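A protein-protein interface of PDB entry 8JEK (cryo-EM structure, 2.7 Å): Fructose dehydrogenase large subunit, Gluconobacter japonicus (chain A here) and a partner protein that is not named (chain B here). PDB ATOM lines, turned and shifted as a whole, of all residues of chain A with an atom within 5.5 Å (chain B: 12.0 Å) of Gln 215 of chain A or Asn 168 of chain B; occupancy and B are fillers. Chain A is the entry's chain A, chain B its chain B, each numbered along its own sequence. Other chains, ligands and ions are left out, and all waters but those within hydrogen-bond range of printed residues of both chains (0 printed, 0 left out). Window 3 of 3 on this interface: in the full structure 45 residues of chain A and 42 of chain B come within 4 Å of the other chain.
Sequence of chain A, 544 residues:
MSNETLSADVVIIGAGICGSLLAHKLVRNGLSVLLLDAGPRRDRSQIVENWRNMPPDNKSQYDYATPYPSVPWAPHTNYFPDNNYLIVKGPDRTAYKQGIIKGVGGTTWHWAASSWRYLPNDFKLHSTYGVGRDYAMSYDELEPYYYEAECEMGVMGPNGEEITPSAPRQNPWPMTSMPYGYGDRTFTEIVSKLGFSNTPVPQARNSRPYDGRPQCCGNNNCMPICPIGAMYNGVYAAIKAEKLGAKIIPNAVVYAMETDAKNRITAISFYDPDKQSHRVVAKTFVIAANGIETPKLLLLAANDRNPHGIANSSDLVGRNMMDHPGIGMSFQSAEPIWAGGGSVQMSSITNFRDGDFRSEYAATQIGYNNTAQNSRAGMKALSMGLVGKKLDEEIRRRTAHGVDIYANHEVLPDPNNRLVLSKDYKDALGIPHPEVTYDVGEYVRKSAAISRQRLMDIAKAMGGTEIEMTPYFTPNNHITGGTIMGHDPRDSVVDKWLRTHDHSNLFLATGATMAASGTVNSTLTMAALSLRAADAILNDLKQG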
ATOM      1  N   MET A 178      15.135 -23.764   7.436  1.00  0.00           N
ATOM      2  CA  MET A 178      14.538 -22.832   8.369  1.00  0.00           C
ATOM      3  C   MET A 178      15.608 -21.913   8.952  1.00  0.00           C
ATOM      4  O   MET A 178      16.790 -22.262   8.983  1.00  0.00           O
ATOM      5  CB  MET A 178      13.819 -23.589   9.481  1.00  0.00           C
ATOM      6  CG  MET A 178      14.729 -24.457  10.327  1.00  0.00           C
ATOM      7  SD  MET A 178      13.830 -25.386  11.578  1.00  0.00           S
ATOM      8  CE  MET A 178      12.655 -26.245  10.546  1.00  0.00           C
ATOM      9  N   PRO A 179      15.218 -20.724   9.409  1.00  0.00           N
ATOM     10  CA  PRO A 179      16.205 -19.772   9.931  1.00  0.00           C
ATOM     11  C   PRO A 179      16.929 -20.306  11.160  1.00  0.00           C
ATOM     12  O   PRO A 179      16.413 -21.128  11.919  1.00  0.00           O
ATOM     13  CB  PRO A 179      15.363 -18.537  10.274  1.00  0.00           C
ATOM     14  CG  PRO A 179      13.954 -19.019  10.308  1.00  0.00           C
ATOM     15  CD  PRO A 179      13.876 -20.128   9.328  1.00  0.00           C
ATOM     16  N   ASN A 206      10.763 -30.365   8.404  1.00  0.00           N
ATOM     17  CA  ASN A 206       9.722 -29.563   7.766  1.00  0.00           C
ATOM     18  C   ASN A 206       9.917 -28.102   8.148  1.00  0.00           C
ATOM     19  O   ASN A 206       9.624 -27.699   9.275  1.00  0.00           O
ATOM     20  CB  ASN A 206       8.335 -30.056   8.164  1.00  0.00           C
ATOM     21  CG  ASN A 206       7.985 -31.391   7.546  1.00  0.00           C
ATOM     22  OD1 ASN A 206       8.668 -31.870   6.644  1.00  0.00           O
ATOM     23  ND2 ASN A 206       6.912 -31.999   8.026  1.00  0.00           N
ATOM     24  N   SER A 207      10.421 -27.307   7.207  1.00  0.00           N
ATOM     25  CA  SER A 207      10.357 -25.857   7.323  1.00  0.00           C
ATOM     26  C   SER A 207       8.996 -25.316   6.915  1.00  0.00           C
ATOM     27  O   SER A 207       8.748 -24.115   7.051  1.00  0.00           O
ATOM     28  CB  SER A 207      11.451 -25.206   6.478  1.00  0.00           C
ATOM     29  OG  SER A 207      11.199 -25.369   5.097  1.00  0.00           O
ATOM     30  N   ARG A 208       8.128 -26.185   6.410  1.00  0.00           N
ATOM     31  CA  ARG A 208       6.735 -25.889   6.122  1.00  0.00           C
ATOM     32  C   ARG A 208       5.976 -27.205   6.145  1.00  0.00           C
ATOM     33  O   ARG A 208       6.589 -28.272   6.030  1.00  0.00           O
ATOM     34  CB  ARG A 208       6.584 -25.196   4.758  1.00  0.00           C
ATOM     35  CG  ARG A 208       7.072 -26.026   3.589  1.00  0.00           C
ATOM     36  CD  ARG A 208       6.703 -25.390   2.265  1.00  0.00           C
ATOM     37  NE  ARG A 208       7.369 -26.045   1.149  1.00  0.00           N
ATOM     38  CZ  ARG A 208       6.930 -27.147   0.558  1.00  0.00           C
ATOM     39  NH1 ARG A 208       5.816 -27.742   0.946  1.00  0.00           N
ATOM     40  NH2 ARG A 208       7.627 -27.664  -0.449  1.00  0.00           N
ATOM     41  N   PRO A 209       4.657 -27.172   6.328  1.00  0.00           N
ATOM     42  CA  PRO A 209       3.891 -28.425   6.311  1.00  0.00           C
ATOM     43  C   PRO A 209       4.140 -29.201   5.026  1.00  0.00           C
ATOM     44  O   PRO A 209       4.070 -28.654   3.924  1.00  0.00           O
ATOM     45  CB  PRO A 209       2.440 -27.950   6.423  1.00  0.00           C
ATOM     46  CG  PRO A 209       2.539 -26.675   7.166  1.00  0.00           C
ATOM     47  CD  PRO A 209       3.812 -26.025   6.705  1.00  0.00           C
ATOM     48  N   ARG A 213       2.372 -33.717   7.333  1.00  0.00           N
ATOM     49  CA  ARG A 213       2.997 -33.643   8.638  1.00  0.00           C
ATOM     50  C   ARG A 213       3.292 -32.192   8.997  1.00  0.00           C
ATOM     51  O   ARG A 213       3.469 -31.354   8.108  1.00  0.00           O
ATOM     52  CB  ARG A 213       4.293 -34.462   8.662  1.00  0.00           C
ATOM     53  CG  ARG A 213       4.067 -35.952   8.478  1.00  0.00           C
ATOM     54  CD  ARG A 213       5.376 -36.703   8.478  1.00  0.00           C
ATOM     55  NE  ARG A 213       6.071 -36.600   7.202  1.00  0.00           N
ATOM     56  CZ  ARG A 213       7.276 -36.072   7.046  1.00  0.00           C
ATOM     57  NH1 ARG A 213       7.943 -35.558   8.064  1.00  0.00           N
ATOM     58  NH2 ARG A 213       7.826 -36.056   5.836  1.00  0.00           N
ATOM     59  N   PRO A 214       3.339 -31.862  10.286  1.00  0.00           N
ATOM     60  CA  PRO A 214       3.439 -30.455  10.688  1.00  0.00           C
ATOM     61  C   PRO A 214       4.803 -29.861  10.373  1.00  0.00           C
ATOM     62  O   PRO A 214       5.782 -30.555  10.099  1.00  0.00           O
ATOM     63  CB  PRO A 214       3.198 -30.509  12.197  1.00  0.00           C
ATOM     64  CG  PRO A 214       3.647 -31.863  12.583  1.00  0.00           C
ATOM     65  CD  PRO A 214       3.227 -32.749  11.456  1.00  0.00           C
ATOM     66  N   GLN A 215       4.843 -28.534  10.405  1.00  0.00           N
ATOM     67  CA  GLN A 215       6.094 -27.798  10.349  1.00  0.00           C
ATOM     68  C   GLN A 215       6.824 -27.914  11.682  1.00  0.00           C
ATOM     69  O   GLN A 215       6.206 -27.997  12.746  1.00  0.00           O
ATOM     70  CB  GLN A 215       5.830 -26.331  10.010  1.00  0.00           C
ATOM     71  CG  GLN A 215       7.066 -25.465   9.910  1.00  0.00           C
ATOM     72  CD  GLN A 215       6.734 -24.013   9.654  1.00  0.00           C
ATOM     73  OE1 GLN A 215       5.605 -23.678   9.306  1.00  0.00           O
ATOM     74  NE2 GLN A 215       7.716 -23.142   9.830  1.00  0.00           N
ATOM     75  N   CYS A 216       8.152 -27.924  11.614  1.00  0.00           N
ATOM     76  CA  CYS A 216       8.971 -28.087  12.808  1.00  0.00           C
ATOM     77  C   CYS A 216       8.816 -26.878  13.724  1.00  0.00           C
ATOM     78  O   CYS A 216       9.059 -25.741  13.311  1.00  0.00           O
ATOM     79  CB  CYS A 216      10.431 -28.286  12.411  1.00  0.00           C
ATOM     80  SG  CYS A 216      11.615 -28.235  13.767  1.00  0.00           S
ATOM     81  N   CYS A 217       8.416 -27.128  14.970  1.00  0.00           N
ATOM     82  CA  CYS A 217       8.259 -26.084  15.973  1.00  0.00           C
ATOM     83  C   CYS A 217       9.464 -25.969  16.895  1.00  0.00           C
ATOM     84  O   CYS A 217       9.370 -25.309  17.933  1.00  0.00           O
ATOM     85  CB  CYS A 217       6.995 -26.323  16.801  1.00  0.00           C
ATOM     86  SG  CYS A 217       6.947 -27.872  17.716  1.00  0.00           S
ATOM     87  N   ILE A 228       5.944 -34.650  17.389  1.00  0.00           N
ATOM     88  CA  ILE A 228       4.903 -34.187  16.479  1.00  0.00           C
ATOM     89  C   ILE A 228       5.057 -34.718  15.063  1.00  0.00           C
ATOM     90  O   ILE A 228       4.138 -34.537  14.253  1.00  0.00           O
ATOM     91  CB  ILE A 228       4.824 -32.645  16.458  1.00  0.00           C
ATOM     92  CG1 ILE A 228       6.000 -32.053  15.684  1.00  0.00           C
ATOM     93  CG2 ILE A 228       4.800 -32.100  17.871  1.00  0.00           C
ATOM     94  CD1 ILE A 228       5.845 -30.582  15.383  1.00  0.00           C
ATOM     95  N   ALA A 230       7.409 -33.802  12.762  1.00  0.00           N
ATOM     96  CA  ALA A 230       7.899 -32.785  11.846  1.00  0.00           C
ATOM     97  C   ALA A 230       9.247 -33.145  11.241  1.00  0.00           C
ATOM     98  O   ALA A 230       9.950 -32.264  10.735  1.00  0.00           O
ATOM     99  CB  ALA A 230       7.989 -31.440  12.559  1.00  0.00           C
ATOM    100  N   VAL B 156      13.552 -18.546  27.565  1.00  0.00           N
ATOM    101  CA  VAL B 156      14.370 -18.548  26.359  1.00  0.00           C
ATOM    102  C   VAL B 156      14.541 -19.956  25.805  1.00  0.00           C
ATOM    103  O   VAL B 156      14.343 -20.193  24.610  1.00  0.00           O
ATOM    104  CB  VAL B 156      15.747 -17.896  26.614  1.00  0.00           C
ATOM    105  CG1 VAL B 156      16.579 -17.915  25.350  1.00  0.00           C
ATOM    106  CG2 VAL B 156      15.580 -16.477  27.122  1.00  0.00           C
ATOM    107  N   VAL B 158      13.998 -24.073  25.317  1.00  0.00           N
ATOM    108  CA  VAL B 158      12.879 -24.998  25.223  1.00  0.00           C
ATOM    109  C   VAL B 158      13.060 -26.140  26.215  1.00  0.00           C
ATOM    110  O   VAL B 158      14.184 -26.582  26.489  1.00  0.00           O
ATOM    111  CB  VAL B 158      12.757 -25.519  23.779  1.00  0.00           C
ATOM    112  CG1 VAL B 158      13.974 -26.344  23.396  1.00  0.00           C
ATOM    113  CG2 VAL B 158      11.496 -26.328  23.599  1.00  0.00           C
ATOM    114  N   PRO B 160      12.518 -29.734  25.940  1.00  0.00           N
ATOM    115  CA  PRO B 160      12.466 -30.310  24.588  1.00  0.00           C
ATOM    116  C   PRO B 160      11.134 -30.858  24.090  1.00  0.00           C
ATOM    117  O   PRO B 160      10.615 -30.358  23.090  1.00  0.00           O
ATOM    118  CB  PRO B 160      13.516 -31.419  24.677  1.00  0.00           C
ATOM    119  CG  PRO B 160      14.561 -30.805  25.538  1.00  0.00           C
ATOM    120  CD  PRO B 160      13.807 -30.021  26.594  1.00  0.00           C
ATOM    121  N   THR B 161      10.547 -31.830  24.759  1.00  0.00           N
ATOM    122  CA  THR B 161       9.376 -32.410  24.089  1.00  0.00           C
ATOM    123  C   THR B 161       8.138 -31.510  24.116  1.00  0.00           C
ATOM    124  O   THR B 161       7.083 -31.942  23.640  1.00  0.00           O
ATOM    125  CB  THR B 161       9.043 -33.768  24.699  1.00  0.00           C
ATOM    126  OG1 THR B 161       9.314 -33.738  26.105  1.00  0.00           O
ATOM    127  CG2 THR B 161       9.854 -34.866  24.032  1.00  0.00           C
ATOM    128  N   TYR B 162       8.233 -30.295  24.644  1.00  0.00           N
ATOM    129  CA  TYR B 162       7.147 -29.330  24.632  1.00  0.00           C
ATOM    130  C   TYR B 162       7.598 -28.102  23.857  1.00  0.00           C
ATOM    131  O   TYR B 162       8.775 -27.742  23.872  1.00  0.00           O
ATOM    132  CB  TYR B 162       6.726 -28.947  26.051  1.00  0.00           C
ATOM    133  CG  TYR B 162       6.250 -30.125  26.867  1.00  0.00           C
ATOM    134  CD1 TYR B 162       7.143 -30.897  27.596  1.00  0.00           C
ATOM    135  CD2 TYR B 162       4.908 -30.476  26.895  1.00  0.00           C
ATOM    136  CE1 TYR B 162       6.713 -31.975  28.335  1.00  0.00           C
ATOM    137  CE2 TYR B 162       4.470 -31.553  27.630  1.00  0.00           C
ATOM    138  CZ  TYR B 162       5.376 -32.299  28.350  1.00  0.00           C
ATOM    139  OH  TYR B 162       4.940 -33.376  29.086  1.00  0.00           O
ATOM    140  N   ALA B 163       6.655 -27.458  23.181  1.00  0.00           N
ATOM    141  CA  ALA B 163       6.969 -26.439  22.189  1.00  0.00           C
ATOM    142  C   ALA B 163       6.932 -25.043  22.794  1.00  0.00           C
ATOM    143  O   ALA B 163       6.005 -24.704  23.537  1.00  0.00           O
ATOM    144  CB  ALA B 163       5.995 -26.518  21.013  1.00  0.00           C
ATOM    145  N   HIS B 164       7.950 -24.246  22.481  1.00  0.00           N
ATOM    146  CA  HIS B 164       7.854 -22.800  22.593  1.00  0.00           C
ATOM    147  C   HIS B 164       6.873 -22.270  21.546  1.00  0.00           C
ATOM    148  O   HIS B 164       6.387 -23.002  20.678  1.00  0.00           O
ATOM    149  CB  HIS B 164       9.229 -22.162  22.407  1.00  0.00           C
ATOM    150  CG  HIS B 164       9.795 -21.537  23.644  1.00  0.00           C
ATOM    151  ND1 HIS B 164       9.815 -20.174  23.845  1.00  0.00           N
ATOM    152  CD2 HIS B 164      10.374 -22.086  24.735  1.00  0.00           C
ATOM    153  CE1 HIS B 164      10.379 -19.911  25.010  1.00  0.00           C
ATOM    154  NE2 HIS B 164      10.725 -21.054  25.571  1.00  0.00           N
ATOM    155  N   ASN B 165       6.596 -20.972  21.611  1.00  0.00           N
ATOM    156  CA  ASN B 165       5.508 -20.420  20.813  1.00  0.00           C
ATOM    157  C   ASN B 165       5.841 -20.326  19.327  1.00  0.00           C
ATOM    158  O   ASN B 165       6.452 -19.352  18.881  1.00  0.00           O
ATOM    159  CB  ASN B 165       5.105 -19.043  21.347  1.00  0.00           C
ATOM    160  CG  ASN B 165       6.280 -18.108  21.504  1.00  0.00           C
ATOM    161  OD1 ASN B 165       7.431 -18.505  21.335  1.00  0.00           O
ATOM    162  ND2 ASN B 165       5.995 -16.854  21.821  1.00  0.00           N
ATOM    163  N   GLY B 166       5.427 -21.324  18.548  1.00  0.00           N
ATOM    164  CA  GLY B 166       5.438 -21.208  17.109  1.00  0.00           C
ATOM    165  C   GLY B 166       6.610 -21.878  16.421  1.00  0.00           C
ATOM    166  O   GLY B 166       7.696 -22.033  16.987  1.00  0.00           O
ATOM    167  N   PRO B 167       6.403 -22.280  15.163  1.00  0.00           N
ATOM    168  CA  PRO B 167       7.440 -23.016  14.429  1.00  0.00           C
ATOM    169  C   PRO B 167       8.663 -22.201  14.032  1.00  0.00           C
ATOM    170  O   PRO B 167       9.572 -22.771  13.421  1.00  0.00           O
ATOM    171  CB  PRO B 167       6.692 -23.502  13.181  1.00  0.00           C
ATOM    172  CG  PRO B 167       5.291 -23.603  13.616  1.00  0.00           C
ATOM    173  CD  PRO B 167       5.088 -22.424  14.521  1.00  0.00           C
ATOM    174  N   ASN B 168       8.726 -20.898  14.310  1.00  0.00           N
ATOM    175  CA  ASN B 168       9.930 -20.143  13.978  1.00  0.00           C
ATOM    176  C   ASN B 168      10.263 -19.108  15.047  1.00  0.00           C
ATOM    177  O   ASN B 168      10.798 -18.040  14.733  1.00  0.00           O
ATOM    178  CB  ASN B 168       9.800 -19.465  12.614  1.00  0.00           C
ATOM    179  CG  ASN B 168      10.390 -20.294  11.492  1.00  0.00           C
ATOM    180  OD1 ASN B 168      11.276 -21.116  11.713  1.00  0.00           O
ATOM    181  ND2 ASN B 168       9.901 -20.082  10.278  1.00  0.00           N
ATOM    182  N   TYR B 169       9.961 -19.410  16.312  1.00  0.00           N
ATOM    183  CA  TYR B 169      10.102 -18.428  17.381  1.00  0.00           C
ATOM    184  C   TYR B 169      11.542 -17.984  17.599  1.00  0.00           C
ATOM    185  O   TYR B 169      11.766 -16.933  18.208  1.00  0.00           O
ATOM    186  CB  TYR B 169       9.539 -18.998  18.685  1.00  0.00           C
ATOM    187  CG  TYR B 169      10.419 -20.045  19.330  1.00  0.00           C
ATOM    188  CD1 TYR B 169      10.309 -21.382  18.978  1.00  0.00           C
ATOM    189  CD2 TYR B 169      11.358 -19.698  20.294  1.00  0.00           C
ATOM    190  CE1 TYR B 169      11.113 -22.338  19.559  1.00  0.00           C
ATOM    191  CE2 TYR B 169      12.165 -20.647  20.877  1.00  0.00           C
ATOM    192  CZ  TYR B 169      12.038 -21.966  20.508  1.00  0.00           C
ATOM    193  OH  TYR B 169      12.841 -22.916  21.093  1.00  0.00           O
ATOM    194  N   TRP B 170      12.519 -18.748  17.119  1.00  0.00           N
ATOM    195  CA  TRP B 170      13.911 -18.526  17.489  1.00  0.00           C
ATOM    196  C   TRP B 170      14.588 -17.425  16.683  1.00  0.00           C
ATOM    197  O   TRP B 170      15.777 -17.171  16.900  1.00  0.00           O
ATOM    198  CB  TRP B 170      14.704 -19.826  17.348  1.00  0.00           C
ATOM    199  CG  TRP B 170      14.485 -20.540  16.053  1.00  0.00           C
ATOM    200  CD1 TRP B 170      15.109 -20.296  14.868  1.00  0.00           C
ATOM    201  CD2 TRP B 170      13.579 -21.619  15.814  1.00  0.00           C
ATOM    202  NE1 TRP B 170      14.651 -21.157  13.904  1.00  0.00           N
ATOM    203  CE2 TRP B 170      13.709 -21.981  14.461  1.00  0.00           C
ATOM    204  CE3 TRP B 170      12.672 -22.317  16.613  1.00  0.00           C
ATOM    205  CZ2 TRP B 170      12.965 -23.004  13.892  1.00  0.00           C
ATOM    206  CZ3 TRP B 170      11.936 -23.331  16.045  1.00  0.00           C
ATOM    207  CH2 TRP B 170      12.090 -23.670  14.700  1.00  0.00           C
ATOM    208  N   VAL B 171      13.878 -16.767  15.770  1.00  0.00           N
ATOM    209  CA  VAL B 171      14.467 -15.701  14.965  1.00  0.00           C
ATOM    210  C   VAL B 171      14.552 -14.424  15.789  1.00  0.00           C
ATOM    211  O   VAL B 171      15.115 -13.419  15.341  1.00  0.00           O
ATOM    212  CB  VAL B 171      13.665 -15.469  13.673  1.00  0.00           C
ATOM    213  CG1 VAL B 171      13.388 -16.788  12.989  1.00  0.00           C
ATOM    214  CG2 VAL B 171      12.373 -14.738  13.975  1.00  0.00           C
ATOM    215  N   SER B 172      13.992 -14.453  16.993  1.00  0.00           N
ATOM    216  CA  SER B 172      14.040 -13.317  17.898  1.00  0.00           C
ATOM    217  C   SER B 172      15.332 -13.332  18.710  1.00  0.00           C
ATOM    218  O   SER B 172      16.034 -14.341  18.798  1.00  0.00           O
ATOM    219  CB  SER B 172      12.828 -13.325  18.825  1.00  0.00           C
ATOM    220  OG  SER B 172      12.846 -14.458  19.676  1.00  0.00           O
ATOM    221  N   GLU B 173      15.646 -12.185  19.303  1.00  0.00           N
ATOM    222  CA  GLU B 173      16.812 -12.107  20.173  1.00  0.00           C
ATOM    223  C   GLU B 173      16.442 -12.536  21.590  1.00  0.00           C
ATOM    224  O   GLU B 173      15.376 -12.168  22.090  1.00  0.00           O
ATOM    225  CB  GLU B 173      17.375 -10.690  20.199  1.00  0.00           C
ATOM    226  CG  GLU B 173      17.925 -10.216  18.864  1.00  0.00           C
ATOM    227  CD  GLU B 173      19.169 -10.972  18.440  1.00  0.00           C
ATOM    228  OE1 GLU B 173      20.227 -10.780  19.073  1.00  0.00           O
ATOM    229  OE2 GLU B 173      19.087 -11.758  17.474  1.00  0.00           O
ATOM    230  N   PRO B 174      17.296 -13.310  22.250  1.00  0.00           N
ATOM    231  CA  PRO B 174      16.973 -13.791  23.595  1.00  0.00           C
ATOM    232  C   PRO B 174      17.168 -12.711  24.649  1.00  0.00           C
ATOM    233  O   PRO B 174      17.836 -11.697  24.434  1.00  0.00           O
ATOM    234  CB  PRO B 174      17.951 -14.951  23.812  1.00  0.00           C
ATOM    235  CG  PRO B 174      18.991 -14.829  22.746  1.00  0.00           C
ATOM    236  CD  PRO B 174      18.642 -13.713  21.816  1.00  0.00           C
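Gln 215 of chain A touches just these residues of chain B: Pro 167 and Asn 168. Asn 168 of chain B touches two residues of chain A. Of the printed residues of chain B, Met 178 of chain A touches Trp 170 (3.4 Å). No residue of chain B comes within 4 Å of Asn 206 of chain A. No residue of chain B comes within 4 Å of Ser 207 of chain A. No residue of chain B comes within 4 Å of Pro 209 of chain A. No residue of chain B comes within 4 Å of Pro 214 of chain A. Cys 216 of chain A touches two residues of chain B. Of the printed residues of chain A, Gly 166 of chain B touches Cys 217. Of the printed residues of chain A, Pro 167 of chain B touches Gln 215, Cys 216 and Cys 217. Of the printed residues of chain A, Trp 170 of chain B touches Met 178, Pro 179, Cys 216 and Cys 217. The nearest printed residue of chain A that does not touch Gly 166 of chain B is Cys 216 of chain A (5.4 Å).
O of Asn 206 of chain A sits at hydrogen-bond distance from N of Cys 216 of chain A, at 2.8 Å. The backbone carbonyl oxygen of Ser 207 of chain A sits at hydrogen-bond distance from the side-chain amide nitrogen of Gln 215 of chain A (3.1 Å). OG of Ser 172 of chain B lies within hydrogen-bond range of O of Tyr 169 of chain B, at 3.1 Å.
Among the printed residues, merely in contact across the chains: Met 178 of chain A with Trp 170 of chain B, Gln 215 of chain A with Pro 167 of chain B, Cys 217 of chain A with Pro 167 of chain B, Pro 179 of chain A with Val 171 of chain B, Pro 179 of chain A with Asn 168 of chain B, Cys 217 of chain A with Ala 163 of chain B, Cys 217 of chain A with Trp 170 of chain B, Gln 215 of chain A with Asn 168 of chain B, Cys 217 of chain A with Gly 166 of chain B, Cys 217 of chain A with Tyr 169 of chain B and Cys 216 of chain A with Trp 170 of chain B.
Of the 13 printed residues of chain A, 5 touch a printed residue of chain B. Hydrophobic or aromatic side chains of chain A within 4 Å of the printed part of chain B: Met 178 and Pro 179.
NE1 of Trp 170 of chain B sits at hydrogen-bond distance from O of Pro 179 of chain A (2.7 Å). O of Cys 216 of chain A sits close to O of Pro 167 of chain B (3.0 Å).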
